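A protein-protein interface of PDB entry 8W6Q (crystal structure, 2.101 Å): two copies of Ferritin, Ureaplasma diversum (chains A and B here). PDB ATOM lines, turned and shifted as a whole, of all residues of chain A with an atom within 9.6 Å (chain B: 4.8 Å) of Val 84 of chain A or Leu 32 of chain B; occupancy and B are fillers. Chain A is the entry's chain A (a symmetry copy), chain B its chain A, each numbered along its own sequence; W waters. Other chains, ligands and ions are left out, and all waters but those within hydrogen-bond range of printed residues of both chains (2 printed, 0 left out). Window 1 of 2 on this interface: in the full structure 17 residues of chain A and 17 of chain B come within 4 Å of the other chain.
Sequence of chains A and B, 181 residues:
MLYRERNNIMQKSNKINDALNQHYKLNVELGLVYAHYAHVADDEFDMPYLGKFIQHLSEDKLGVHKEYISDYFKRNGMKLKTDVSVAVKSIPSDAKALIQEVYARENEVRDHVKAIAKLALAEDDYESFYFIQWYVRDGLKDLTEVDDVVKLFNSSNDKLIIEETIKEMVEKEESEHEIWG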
ATOM      1  N   ASN A  21      -9.649  26.366 -11.456  1.00  0.00           N
ATOM      2  CA  ASN A  21      -9.898  25.156 -10.672  1.00  0.00           C
ATOM      3  C   ASN A  21      -8.887  24.079 -11.019  1.00  0.00           C
ATOM      4  O   ASN A  21      -8.432  23.337 -10.142  1.00  0.00           O
ATOM      5  CB  ASN A  21     -11.314  24.637 -10.914  1.00  0.00           C
ATOM      6  CG  ASN A  21     -12.301  25.156  -9.893  1.00  0.00           C
ATOM      7  OD1 ASN A  21     -12.002  25.214  -8.709  1.00  0.00           O
ATOM      8  ND2 ASN A  21     -13.498  25.503 -10.347  1.00  0.00           N
ATOM      9  N   GLN A  22      -8.526  23.978 -12.300  1.00  0.00           N
ATOM     10  CA  GLN A  22      -7.483  23.043 -12.702  1.00  0.00           C
ATOM     11  C   GLN A  22      -6.146  23.432 -12.076  1.00  0.00           C
ATOM     12  O   GLN A  22      -5.382  22.574 -11.623  1.00  0.00           O
ATOM     13  CB  GLN A  22      -7.389  23.021 -14.232  1.00  0.00           C
ATOM     14  CG  GLN A  22      -6.465  21.982 -14.824  1.00  0.00           C
ATOM     15  CD  GLN A  22      -6.150  22.270 -16.289  1.00  0.00           C
ATOM     16  OE1 GLN A  22      -7.001  22.759 -17.040  1.00  0.00           O
ATOM     17  NE2 GLN A  22      -4.929  21.949 -16.703  1.00  0.00           N
ATOM     18  N   HIS A  23      -5.852  24.728 -12.020  1.00  0.00           N
ATOM     19  CA  HIS A  23      -4.611  25.163 -11.387  1.00  0.00           C
ATOM     20  C   HIS A  23      -4.639  24.964  -9.867  1.00  0.00           C
ATOM     21  O   HIS A  23      -3.615  24.624  -9.264  1.00  0.00           O
ATOM     22  CB  HIS A  23      -4.322  26.619 -11.739  1.00  0.00           C
ATOM     23  CG  HIS A  23      -2.868  26.948 -11.670  1.00  0.00           C
ATOM     24  ND1 HIS A  23      -1.932  26.309 -12.456  1.00  0.00           N
ATOM     25  CD2 HIS A  23      -2.173  27.750 -10.832  1.00  0.00           C
ATOM     26  CE1 HIS A  23      -0.728  26.760 -12.153  1.00  0.00           C
ATOM     27  NE2 HIS A  23      -0.845  27.631 -11.167  1.00  0.00           N
ATOM     28  N   TYR A  24      -5.792  25.162  -9.229  1.00  0.00           N
ATOM     29  CA  TYR A  24      -5.948  24.778  -7.822  1.00  0.00           C
ATOM     30  C   TYR A  24      -5.618  23.300  -7.621  1.00  0.00           C
ATOM     31  O   TYR A  24      -4.858  22.927  -6.717  1.00  0.00           O
ATOM     32  CB  TYR A  24      -7.387  25.075  -7.377  1.00  0.00           C
ATOM     33  CG  TYR A  24      -7.697  24.863  -5.908  1.00  0.00           C
ATOM     34  CD1 TYR A  24      -8.122  23.624  -5.432  1.00  0.00           C
ATOM     35  CD2 TYR A  24      -7.617  25.917  -5.004  1.00  0.00           C
ATOM     36  CE1 TYR A  24      -8.416  23.430  -4.076  1.00  0.00           C
ATOM     37  CE2 TYR A  24      -7.909  25.729  -3.646  1.00  0.00           C
ATOM     38  CZ  TYR A  24      -8.310  24.487  -3.197  1.00  0.00           C
ATOM     39  OH  TYR A  24      -8.611  24.301  -1.863  1.00  0.00           O
ATOM     40  N   LYS A  25      -6.183  22.446  -8.474  1.00  0.00           N
ATOM     41  CA  LYS A  25      -5.942  21.010  -8.398  1.00  0.00           C
ATOM     42  C   LYS A  25      -4.460  20.678  -8.558  1.00  0.00           C
ATOM     43  O   LYS A  25      -3.898  19.889  -7.789  1.00  0.00           O
ATOM     44  CB  LYS A  25      -6.772  20.327  -9.482  1.00  0.00           C
ATOM     45  CG  LYS A  25      -6.483  18.845  -9.729  1.00  0.00           C
ATOM     46  CD  LYS A  25      -7.436  18.331 -10.831  1.00  0.00           C
ATOM     47  CE  LYS A  25      -7.063  16.938 -11.304  1.00  0.00           C
ATOM     48  NZ  LYS A  25      -7.655  15.910 -10.417  1.00  0.00           N
ATOM     49  N   LEU A  26      -3.823  21.247  -9.582  1.00  0.00           N
ATOM     50  CA  LEU A  26      -2.402  21.016  -9.810  1.00  0.00           C
ATOM     51  C   LEU A  26      -1.582  21.377  -8.579  1.00  0.00           C
ATOM     52  O   LEU A  26      -0.667  20.639  -8.195  1.00  0.00           O
ATOM     53  CB  LEU A  26      -1.944  21.839 -11.019  1.00  0.00           C
ATOM     54  CG  LEU A  26      -0.550  21.659 -11.657  1.00  0.00           C
ATOM     55  CD1 LEU A  26      -0.472  22.488 -12.922  1.00  0.00           C
ATOM     56  CD2 LEU A  26       0.579  22.076 -10.735  1.00  0.00           C
ATOM     57  N   ASN A  27      -1.880  22.523  -7.957  1.00  0.00           N
ATOM     58  CA  ASN A  27      -1.073  22.961  -6.820  1.00  0.00           C
ATOM     59  C   ASN A  27      -1.268  22.067  -5.603  1.00  0.00           C
ATOM     60  O   ASN A  27      -0.322  21.838  -4.839  1.00  0.00           O
ATOM     61  CB  ASN A  27      -1.391  24.405  -6.480  1.00  0.00           C
ATOM     62  CG  ASN A  27      -0.569  25.353  -7.294  1.00  0.00           C
ATOM     63  OD1 ASN A  27       0.608  25.538  -7.022  1.00  0.00           O
ATOM     64  ND2 ASN A  27      -1.173  25.949  -8.307  1.00  0.00           N
ATOM     65  N   VAL A  28      -2.485  21.560  -5.398  1.00  0.00           N
ATOM     66  CA  VAL A  28      -2.688  20.584  -4.333  1.00  0.00           C
ATOM     67  C   VAL A  28      -1.873  19.329  -4.618  1.00  0.00           C
ATOM     68  O   VAL A  28      -1.091  18.865  -3.781  1.00  0.00           O
ATOM     69  CB  VAL A  28      -4.181  20.252  -4.178  1.00  0.00           C
ATOM     70  CG1 VAL A  28      -4.347  19.033  -3.262  1.00  0.00           C
ATOM     71  CG2 VAL A  28      -4.935  21.455  -3.632  1.00  0.00           C
ATOM     72  N   GLU A  29      -2.013  18.791  -5.834  1.00  0.00           N
ATOM     73  CA  GLU A  29      -1.409  17.506  -6.136  1.00  0.00           C
ATOM     74  C   GLU A  29       0.110  17.611  -6.190  1.00  0.00           C
ATOM     75  O   GLU A  29       0.811  16.737  -5.670  1.00  0.00           O
ATOM     76  CB  GLU A  29      -2.012  16.960  -7.433  1.00  0.00           C
ATOM     77  CG  GLU A  29      -3.463  16.508  -7.194  1.00  0.00           C
ATOM     78  CD  GLU A  29      -4.238  16.195  -8.459  1.00  0.00           C
ATOM     79  OE1 GLU A  29      -5.440  15.887  -8.336  1.00  0.00           O
ATOM     80  OE2 GLU A  29      -3.665  16.249  -9.570  1.00  0.00           O
ATOM     81  N   LEU A  30       0.635  18.685  -6.788  1.00  0.00           N
ATOM     82  CA  LEU A  30       2.070  18.958  -6.717  1.00  0.00           C
ATOM     83  C   LEU A  30       2.552  19.012  -5.273  1.00  0.00           C
ATOM     84  O   LEU A  30       3.567  18.395  -4.915  1.00  0.00           O
ATOM     85  CB  LEU A  30       2.383  20.286  -7.413  1.00  0.00           C
ATOM     86  CG  LEU A  30       3.212  20.325  -8.688  1.00  0.00           C
ATOM     87  CD1 LEU A  30       3.576  21.773  -8.992  1.00  0.00           C
ATOM     88  CD2 LEU A  30       4.454  19.478  -8.515  1.00  0.00           C
ATOM     89  N   GLY A  31       1.849  19.778  -4.434  1.00  0.00           N
ATOM     90  CA  GLY A  31       2.269  19.918  -3.050  1.00  0.00           C
ATOM     91  C   GLY A  31       2.349  18.586  -2.334  1.00  0.00           C
ATOM     92  O   GLY A  31       3.249  18.357  -1.523  1.00  0.00           O
ATOM     93  N   LEU A  32       1.428  17.679  -2.650  1.00  0.00           N
ATOM     94  CA  LEU A  32       1.445  16.363  -2.020  1.00  0.00           C
ATOM     95  C   LEU A  32       2.588  15.505  -2.558  1.00  0.00           C
ATOM     96  O   LEU A  32       3.198  14.726  -1.807  1.00  0.00           O
ATOM     97  CB  LEU A  32       0.092  15.678  -2.227  1.00  0.00           C
ATOM     98  CG  LEU A  32      -1.099  16.349  -1.530  1.00  0.00           C
ATOM     99  CD1 LEU A  32      -2.447  15.702  -1.883  1.00  0.00           C
ATOM    100  CD2 LEU A  32      -0.882  16.291  -0.020  1.00  0.00           C
ATOM    101  N   VAL A  33       2.902  15.629  -3.850  1.00  0.00           N
ATOM    102  CA  VAL A  33       4.057  14.921  -4.396  1.00  0.00           C
ATOM    103  C   VAL A  33       5.338  15.463  -3.781  1.00  0.00           C
ATOM    104  O   VAL A  33       6.246  14.702  -3.410  1.00  0.00           O
ATOM    105  CB  VAL A  33       4.085  15.035  -5.933  1.00  0.00           C
ATOM    106  CG1 VAL A  33       5.457  14.634  -6.479  1.00  0.00           C
ATOM    107  CG2 VAL A  33       2.988  14.186  -6.547  1.00  0.00           C
ATOM    108  N   LYS A  61       2.982  25.359  -2.380  1.00  0.00           N
ATOM    109  CA  LYS A  61       1.926  24.921  -3.294  1.00  0.00           C
ATOM    110  C   LYS A  61       0.614  24.710  -2.551  1.00  0.00           C
ATOM    111  O   LYS A  61      -0.445  25.167  -2.993  1.00  0.00           O
ATOM    112  CB  LYS A  61       2.341  23.623  -3.997  1.00  0.00           C
ATOM    113  CG  LYS A  61       3.655  23.661  -4.756  1.00  0.00           C
ATOM    114  CD  LYS A  61       3.733  24.831  -5.730  1.00  0.00           C
ATOM    115  CE  LYS A  61       4.999  24.756  -6.578  1.00  0.00           C
ATOM    116  NZ  LYS A  61       5.029  25.809  -7.646  1.00  0.00           N
ATOM    117  N   LEU A  62       0.667  24.007  -1.425  1.00  0.00           N
ATOM    118  CA  LEU A  62      -0.523  23.764  -0.622  1.00  0.00           C
ATOM    119  C   LEU A  62      -0.920  24.970   0.206  1.00  0.00           C
ATOM    120  O   LEU A  62      -1.951  24.922   0.881  1.00  0.00           O
ATOM    121  CB  LEU A  62      -0.299  22.557   0.285  1.00  0.00           C
ATOM    122  CG  LEU A  62      -0.319  21.192  -0.391  1.00  0.00           C
ATOM    123  CD1 LEU A  62       0.418  20.178   0.469  1.00  0.00           C
ATOM    124  CD2 LEU A  62      -1.753  20.772  -0.600  1.00  0.00           C
ATOM    125  N   GLY A  63      -0.122  26.035   0.176  1.00  0.00           N
ATOM    126  CA  GLY A  63      -0.391  27.233   0.951  1.00  0.00           C
ATOM    127  C   GLY A  63      -0.867  28.360   0.063  1.00  0.00           C
ATOM    128  O   GLY A  63      -1.955  28.258  -0.501  1.00  0.00           O
ATOM    129  N   LYS A  66      -2.638  27.786  -3.586  1.00  0.00           N
ATOM    130  CA  LYS A  66      -4.049  27.438  -3.690  1.00  0.00           C
ATOM    131  C   LYS A  66      -4.917  28.461  -2.976  1.00  0.00           C
ATOM    132  O   LYS A  66      -6.026  28.765  -3.433  1.00  0.00           O
ATOM    133  CB  LYS A  66      -4.318  26.025  -3.138  1.00  0.00           C
ATOM    134  CG  LYS A  66      -4.524  25.901  -1.605  1.00  0.00           C
ATOM    135  CD  LYS A  66      -4.702  24.438  -1.197  1.00  0.00           C
ATOM    136  CE  LYS A  66      -5.403  24.296   0.156  1.00  0.00           C
ATOM    137  NZ  LYS A  66      -4.698  25.076   1.215  1.00  0.00           N
ATOM    138  N   LEU A  80     -15.561  27.213  -6.526  1.00  0.00           N
ATOM    139  CA  LEU A  80     -14.437  26.338  -6.200  1.00  0.00           C
ATOM    140  C   LEU A  80     -14.830  24.870  -6.363  1.00  0.00           C
ATOM    141  O   LEU A  80     -15.914  24.456  -5.943  1.00  0.00           O
ATOM    142  CB  LEU A  80     -13.956  26.584  -4.771  1.00  0.00           C
ATOM    143  CG  LEU A  80     -12.790  25.688  -4.329  1.00  0.00           C
ATOM    144  CD1 LEU A  80     -11.515  26.084  -5.050  1.00  0.00           C
ATOM    145  CD2 LEU A  80     -12.595  25.732  -2.811  1.00  0.00           C
ATOM    146  N   LYS A  81     -13.950  24.084  -6.976  1.00  0.00           N
ATOM    147  CA  LYS A  81     -14.100  22.638  -7.043  1.00  0.00           C
ATOM    148  C   LYS A  81     -12.913  21.985  -6.352  1.00  0.00           C
ATOM    149  O   LYS A  81     -11.764  22.378  -6.582  1.00  0.00           O
ATOM    150  CB  LYS A  81     -14.209  22.148  -8.492  1.00  0.00           C
ATOM    151  CG  LYS A  81     -15.635  22.181  -9.023  1.00  0.00           C
ATOM    152  CD  LYS A  81     -15.745  22.846 -10.393  1.00  0.00           C
ATOM    153  CE  LYS A  81     -16.354  21.902 -11.431  1.00  0.00           C
ATOM    154  NZ  LYS A  81     -16.193  22.422 -12.824  1.00  0.00           N
ATOM    155  N   THR A  82     -13.190  21.003  -5.499  1.00  0.00           N
ATOM    156  CA  THR A  82     -12.149  20.195  -4.865  1.00  0.00           C
ATOM    157  C   THR A  82     -12.280  18.774  -5.399  1.00  0.00           C
ATOM    158  O   THR A  82     -13.271  18.089  -5.122  1.00  0.00           O
ATOM    159  CB  THR A  82     -12.254  20.248  -3.340  1.00  0.00           C
ATOM    160  OG1 THR A  82     -11.932  21.571  -2.897  1.00  0.00           O
ATOM    161  CG2 THR A  82     -11.270  19.283  -2.687  1.00  0.00           C
ATOM    162  N   ASP A  83     -11.287  18.351  -6.187  1.00  0.00           N
ATOM    163  CA  ASP A  83     -11.283  17.034  -6.830  1.00  0.00           C
ATOM    164  C   ASP A  83      -9.815  16.645  -7.008  1.00  0.00           C
ATOM    165  O   ASP A  83      -9.148  17.108  -7.941  1.00  0.00           O
ATOM    166  CB  ASP A  83     -12.037  17.079  -8.159  1.00  0.00           C
ATOM    167  CG  ASP A  83     -12.046  15.741  -8.886  1.00  0.00           C
ATOM    168  OD1 ASP A  83     -11.635  14.717  -8.298  1.00  0.00           O
ATOM    169  OD2 ASP A  83     -12.457  15.722 -10.065  1.00  0.00           O
ATOM    170  N   VAL A  84      -9.315  15.809  -6.105  1.00  0.00           N
ATOM    171  CA  VAL A  84      -7.884  15.566  -5.959  1.00  0.00           C
ATOM    172  C   VAL A  84      -7.625  14.076  -6.076  1.00  0.00           C
ATOM    173  O   VAL A  84      -8.261  13.281  -5.378  1.00  0.00           O
ATOM    174  CB  VAL A  84      -7.363  16.097  -4.607  1.00  0.00           C
ATOM    175  CG1 VAL A  84      -5.897  15.713  -4.394  1.00  0.00           C
ATOM    176  CG2 VAL A  84      -7.560  17.609  -4.523  1.00  0.00           C
ATOM    177  N   SER A  85      -6.695  13.697  -6.949  1.00  0.00           N
ATOM    178  CA  SER A  85      -6.239  12.316  -6.997  1.00  0.00           C
ATOM    179  C   SER A  85      -4.769  12.303  -7.372  1.00  0.00           C
ATOM    180  O   SER A  85      -4.404  12.721  -8.474  1.00  0.00           O
ATOM    181  CB  SER A  85      -7.055  11.484  -7.983  1.00  0.00           C
ATOM    182  OG  SER A  85      -6.706  11.763  -9.313  1.00  0.00           O
ATOM    183  N   VAL A  86      -3.926  11.821  -6.468  1.00  0.00           N
ATOM    184  CA  VAL A  86      -2.521  11.670  -6.794  1.00  0.00           C
ATOM    185  C   VAL A  86      -1.958  10.519  -5.976  1.00  0.00           C
ATOM    186  O   VAL A  86      -2.310  10.332  -4.810  1.00  0.00           O
ATOM    187  CB  VAL A  86      -1.752  12.993  -6.580  1.00  0.00           C
ATOM    188  CG1 VAL A  86      -1.802  13.431  -5.112  1.00  0.00           C
ATOM    189  CG2 VAL A  86      -0.321  12.863  -7.109  1.00  0.00           C
ATOM    190  N   ALA A  87      -1.119   9.714  -6.619  1.00  0.00           N
ATOM    191  CA  ALA A  87      -0.429   8.617  -5.954  1.00  0.00           C
ATOM    192  C   ALA A  87       1.012   8.635  -6.412  1.00  0.00           C
ATOM    193  O   ALA A  87       1.283   8.718  -7.614  1.00  0.00           O
ATOM    194  CB  ALA A  87      -1.068   7.258  -6.270  1.00  0.00           C
ATOM    195  N   VAL B  28      -4.558  14.022   5.198  1.00  0.00           N
ATOM    196  CA  VAL B  28      -4.480  14.787   3.958  1.00  0.00           C
ATOM    197  C   VAL B  28      -5.883  15.057   3.428  1.00  0.00           C
ATOM    198  O   VAL B  28      -6.258  16.202   3.154  1.00  0.00           O
ATOM    199  CB  VAL B  28      -3.626  14.048   2.916  1.00  0.00           C
ATOM    200  CG1 VAL B  28      -3.787  14.718   1.546  1.00  0.00           C
ATOM    201  CG2 VAL B  28      -2.168  14.025   3.348  1.00  0.00           C
ATOM    202  N   GLU B  29      -6.693  13.999   3.322  1.00  0.00           N
ATOM    203  CA  GLU B  29      -7.985  14.133   2.671  1.00  0.00           C
ATOM    204  C   GLU B  29      -8.939  14.974   3.509  1.00  0.00           C
ATOM    205  O   GLU B  29      -9.655  15.823   2.967  1.00  0.00           O
ATOM    206  CB  GLU B  29      -8.537  12.739   2.361  1.00  0.00           C
ATOM    207  CG  GLU B  29      -7.740  12.095   1.215  1.00  0.00           C
ATOM    208  CD  GLU B  29      -8.030  10.622   1.001  1.00  0.00           C
ATOM    209  OE1 GLU B  29      -7.366  10.026   0.129  1.00  0.00           O
ATOM    210  OE2 GLU B  29      -8.909  10.054   1.686  1.00  0.00           O
ATOM    211  N   LEU B  30      -8.943  14.774   4.829  1.00  0.00           N
ATOM    212  CA  LEU B  30      -9.685  15.664   5.722  1.00  0.00           C
ATOM    213  C   LEU B  30      -9.269  17.116   5.526  1.00  0.00           C
ATOM    214  O   LEU B  30     -10.118  18.012   5.399  1.00  0.00           O
ATOM    215  CB  LEU B  30      -9.450  15.256   7.180  1.00  0.00           C
ATOM    216  CG  LEU B  30     -10.584  14.705   8.030  1.00  0.00           C
ATOM    217  CD1 LEU B  30     -10.123  14.641   9.481  1.00  0.00           C
ATOM    218  CD2 LEU B  30     -11.805  15.587   7.887  1.00  0.00           C
ATOM    219  N   GLY B  31      -7.957  17.371   5.531  1.00  0.00           N
ATOM    220  CA  GLY B  31      -7.480  18.737   5.394  1.00  0.00           C
ATOM    221  C   GLY B  31      -7.964  19.391   4.118  1.00  0.00           C
ATOM    222  O   GLY B  31      -8.292  20.580   4.101  1.00  0.00           O
ATOM    223  N   LEU B  32      -8.047  18.615   3.039  1.00  0.00           N
ATOM    224  CA  LEU B  32      -8.521  19.162   1.773  1.00  0.00           C
ATOM    225  C   LEU B  32     -10.028  19.411   1.806  1.00  0.00           C
ATOM    226  O   LEU B  32     -10.517  20.392   1.223  1.00  0.00           O
ATOM    227  CB  LEU B  32      -8.139  18.218   0.631  1.00  0.00           C
ATOM    228  CG  LEU B  32      -6.634  18.075   0.370  1.00  0.00           C
ATOM    229  CD1 LEU B  32      -6.304  17.014  -0.691  1.00  0.00           C
ATOM    230  CD2 LEU B  32      -6.080  19.428  -0.067  1.00  0.00           C
ATOM    231  N   VAL B  33     -10.785  18.543   2.483  1.00  0.00           N
ATOM    232  CA  VAL B  33     -12.215  18.790   2.646  1.00  0.00           C
ATOM    233  C   VAL B  33     -12.436  20.026   3.503  1.00  0.00           C
ATOM    234  O   VAL B  33     -13.293  20.872   3.204  1.00  0.00           O
ATOM    235  CB  VAL B  33     -12.911  17.556   3.256  1.00  0.00           C
ATOM    236  CG1 VAL B  33     -14.303  17.923   3.774  1.00  0.00           C
ATOM    237  CG2 VAL B  33     -12.988  16.434   2.238  1.00  0.00           C
ATOM    238  N   TYR B  34     -11.674  20.152   4.588  1.00  0.00           N
ATOM    239  CA  TYR B  34     -11.837  21.324   5.440  1.00  0.00           C
ATOM    240  C   TYR B  34     -11.482  22.606   4.698  1.00  0.00           C
ATOM    241  O   TYR B  34     -12.106  23.644   4.930  1.00  0.00           O
ATOM    242  CB  TYR B  34     -10.989  21.189   6.702  1.00  0.00           C
ATOM    243  CG  TYR B  34     -11.493  20.170   7.689  1.00  0.00           C
ATOM    244  CD1 TYR B  34     -12.736  19.573   7.533  1.00  0.00           C
ATOM    245  CD2 TYR B  34     -10.727  19.812   8.789  1.00  0.00           C
ATOM    246  CE1 TYR B  34     -13.195  18.631   8.446  1.00  0.00           C
ATOM    247  CE2 TYR B  34     -11.183  18.883   9.710  1.00  0.00           C
ATOM    248  CZ  TYR B  34     -12.418  18.304   9.535  1.00  0.00           C
ATOM    249  OH  TYR B  34     -12.865  17.373  10.441  1.00  0.00           O
ATOM    250  N   ALA B  35     -10.486  22.561   3.804  1.00  0.00           N
ATOM    251  CA  ALA B  35     -10.172  23.754   3.028  1.00  0.00           C
ATOM    252  C   ALA B  35     -11.364  24.150   2.168  1.00  0.00           C
ATOM    253  O   ALA B  35     -11.657  25.339   2.006  1.00  0.00           O
ATOM    254  CB  ALA B  35      -8.937  23.525   2.152  1.00  0.00           C
ATOM    255  N   HIS B  36     -12.069  23.160   1.616  1.00  0.00           N
ATOM    256  CA  HIS B  36     -13.271  23.458   0.843  1.00  0.00           C
ATOM    257  C   HIS B  36     -14.381  23.985   1.742  1.00  0.00           C
ATOM    258  O   HIS B  36     -15.002  25.010   1.440  1.00  0.00           O
ATOM    259  CB  HIS B  36     -13.739  22.214   0.101  1.00  0.00           C
ATOM    260  CG  HIS B  36     -14.664  22.520  -1.027  1.00  0.00           C
ATOM    261  ND1 HIS B  36     -16.006  22.778  -0.835  1.00  0.00           N
ATOM    262  CD2 HIS B  36     -14.443  22.636  -2.356  1.00  0.00           C
ATOM    263  CE1 HIS B  36     -16.572  23.030  -2.002  1.00  0.00           C
ATOM    264  NE2 HIS B  36     -15.646  22.948  -2.942  1.00  0.00           N
ATOM    265  N   SER B  58      -8.013  22.894   8.766  1.00  0.00           N
ATOM    266  CA  SER B  58      -7.415  22.394   7.528  1.00  0.00           C
ATOM    267  C   SER B  58      -5.897  22.358   7.625  1.00  0.00           C
ATOM    268  O   SER B  58      -5.259  21.352   7.295  1.00  0.00           O
ATOM    269  CB  SER B  58      -7.846  23.265   6.346  1.00  0.00           C
ATOM    270  OG  SER B  58      -7.298  22.754   5.137  1.00  0.00           O
ATOM    271  N   LEU B  62      -3.261  19.038   7.404  1.00  0.00           N
ATOM    272  CA  LEU B  62      -2.240  18.999   6.368  1.00  0.00           C
ATOM    273  C   LEU B  62      -0.876  19.415   6.883  1.00  0.00           C
ATOM    274  O   LEU B  62       0.095  19.361   6.124  1.00  0.00           O
ATOM    275  CB  LEU B  62      -2.652  19.890   5.199  1.00  0.00           C
ATOM    276  CG  LEU B  62      -3.763  19.357   4.304  1.00  0.00           C
ATOM    277  CD1 LEU B  62      -4.420  20.506   3.555  1.00  0.00           C
ATOM    278  CD2 LEU B  62      -3.174  18.359   3.338  1.00  0.00           C
ATOM    279  N   VAL B  84      -3.807   9.574  -2.541  1.00  0.00           N
ATOM    280  CA  VAL B  84      -4.811  10.533  -2.093  1.00  0.00           C
ATOM    281  C   VAL B  84      -5.907  10.620  -3.139  1.00  0.00           C
ATOM    282  O   VAL B  84      -5.619  10.830  -4.321  1.00  0.00           O
ATOM    283  CB  VAL B  84      -4.187  11.924  -1.854  1.00  0.00           C
ATOM    284  CG1 VAL B  84      -5.264  12.961  -1.527  1.00  0.00           C
ATOM    285  CG2 VAL B  84      -3.135  11.847  -0.750  1.00  0.00           C
ATOM    286  N   SER B  85      -7.157  10.462  -2.710  1.00  0.00           N
ATOM    287  CA  SER B  85      -8.284  10.717  -3.595  1.00  0.00           C
ATOM    288  C   SER B  85      -9.431  11.271  -2.771  1.00  0.00           C
ATOM    289  O   SER B  85      -9.958  10.582  -1.893  1.00  0.00           O
ATOM    290  CB  SER B  85      -8.715   9.457  -4.341  1.00  0.00           C
ATOM    291  OG  SER B  85      -9.423   8.576  -3.510  1.00  0.00           O
ATOM    292  N   VAL B  86      -9.824  12.508  -3.051  1.00  0.00           N
ATOM    293  CA  VAL B  86     -10.987  13.067  -2.387  1.00  0.00           C
ATOM    294  C   VAL B  86     -11.630  14.082  -3.317  1.00  0.00           C
ATOM    295  O   VAL B  86     -10.946  14.827  -4.021  1.00  0.00           O
ATOM    296  CB  VAL B  86     -10.611  13.663  -1.012  1.00  0.00           C
ATOM    297  CG1 VAL B  86      -9.614  14.816  -1.162  1.00  0.00           C
ATOM    298  CG2 VAL B  86     -11.876  14.072  -0.251  1.00  0.00           C
HETATM  299  O   HOH W   1      -5.357  24.084   3.707  1.00  0.00           O
HETATM  300  O   HOH W   2      -9.903  22.013  -1.173  1.00  0.00           O
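The backbone carbonyl oxygen (O) of Val 86 of chain A sits at hydrogen-bond distance from the backbone NH (N) of Val 84 of chain B, at 2.8 Å. O of Val 86 of chain B lies within hydrogen-bond range of N of Val 84 of chain A, 2.8 Å away. NE2 of His 36 of chain B is in hydrogen-bond range of O of Leu 80 of chain A, 3.4 Å away.
The side-chain carboxylate (OE1) of Glu 29 of chain A is in hydrogen-bond range of the backbone NH (N) of Ser 85 of chain A (2.9 Å). NZ of Lys 25 of chain A lies within hydrogen-bond range of O of Asp 83 of chain A (3.1 Å). OE1 of Glu 29 of chain B sits at hydrogen-bond distance from N of Ser 85 of chain B, at 2.9 Å.
CG1 of Val 28 of chain A touches CD2 of Leu 32 of chain B (3.7 Å). CD2 of Leu 32 of chain A touches CG1 of Val 28 of chain B, 3.7 Å away. Leu 32 of chain A touches Val 84 of chain B (CD1 to CG1, 3.9 Å). CD2 of His 36 of chain B touches OG1 of Thr 82 of chain A (2.8 Å). Asp 83 of chain A touches Val 86 of chain B. Leu 32 of chain B touches Val 84 of chain A. O of Val 84 of chain A touches O of Val 84 of chain B, 3.8 Å away. O of Val 84 of chain A touches CA of Ser 85 of chain B, at 3.1 Å. O of Val 84 of chain B touches CA of Ser 85 of chain A, at 3.1 Å.
Of the printed residues of chain B, Thr 82 of chain A touches His 36 (2.8 Å). Printed residues of chain B within 4 Å of Asp 83 of chain A: Val 86. Val 84 of chain A touches just these residues of chain B: Leu 32, Val 84, Ser 85 and Val 86. Printed residues of chain B within 4 Å of Val 86 of chain A: Val 84 (2.8 Å). Of the printed residues of chain A, Val 28 of chain B touches Leu 32 (3.7 Å). Of chain A, only Val 28 (3.7 Å) and Val 84 (3.9 Å) come within 4 Å of Leu 32 of chain B. Of the printed residues of chain A, His 36 of chain B touches Leu 80 (3.4 Å) and Thr 82 (2.8 Å). The nearest printed residue of chain B that does not touch Val 84 of chain A is Val 28 of chain B (6.4 Å).
Of the 14 printed residues of chain B, 6 touch a printed residue of chain A. Along chain B the printed residues that touch a printed residue of chain A span positions 28 to 86. Of the 25 printed residues of chain A, 8 touch a printed residue of chain B. Along chain A the printed residues that touch a printed residue of chain B span positions 28 to 86. Among the printed residues, 12 pairs touch across the chains.
Val 28 of chain A touches Leu 32 of chain B, and with the chains exchanged Leu 32 of chain A touches Val 28 of chain B. Leu 32 of chain A touches Val 84 of chain B, and with the chains exchanged Val 84 of chain A touches Leu 32 of chain B. Val 84 of chain A touches its own counterpart, Val 84 of chain B. Val 84 of chain A touches Val 86 of chain B, and with the chains exchanged Val 86 of chain A touches Val 84 of chain B.
Water W2 lies within hydrogen-bond range of OG1 of Thr 82 of chain A (2.7 Å), OH of Tyr 24 of chain A (2.7 Å) and O of Leu 32 of chain B (3.0 Å). Water W1 lies within hydrogen-bond range of the side-chain hydroxyl of Ser 58 of chain B (2.8 Å) and the side-chain amino group of Lys 66 of chain A (2.8 Å).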
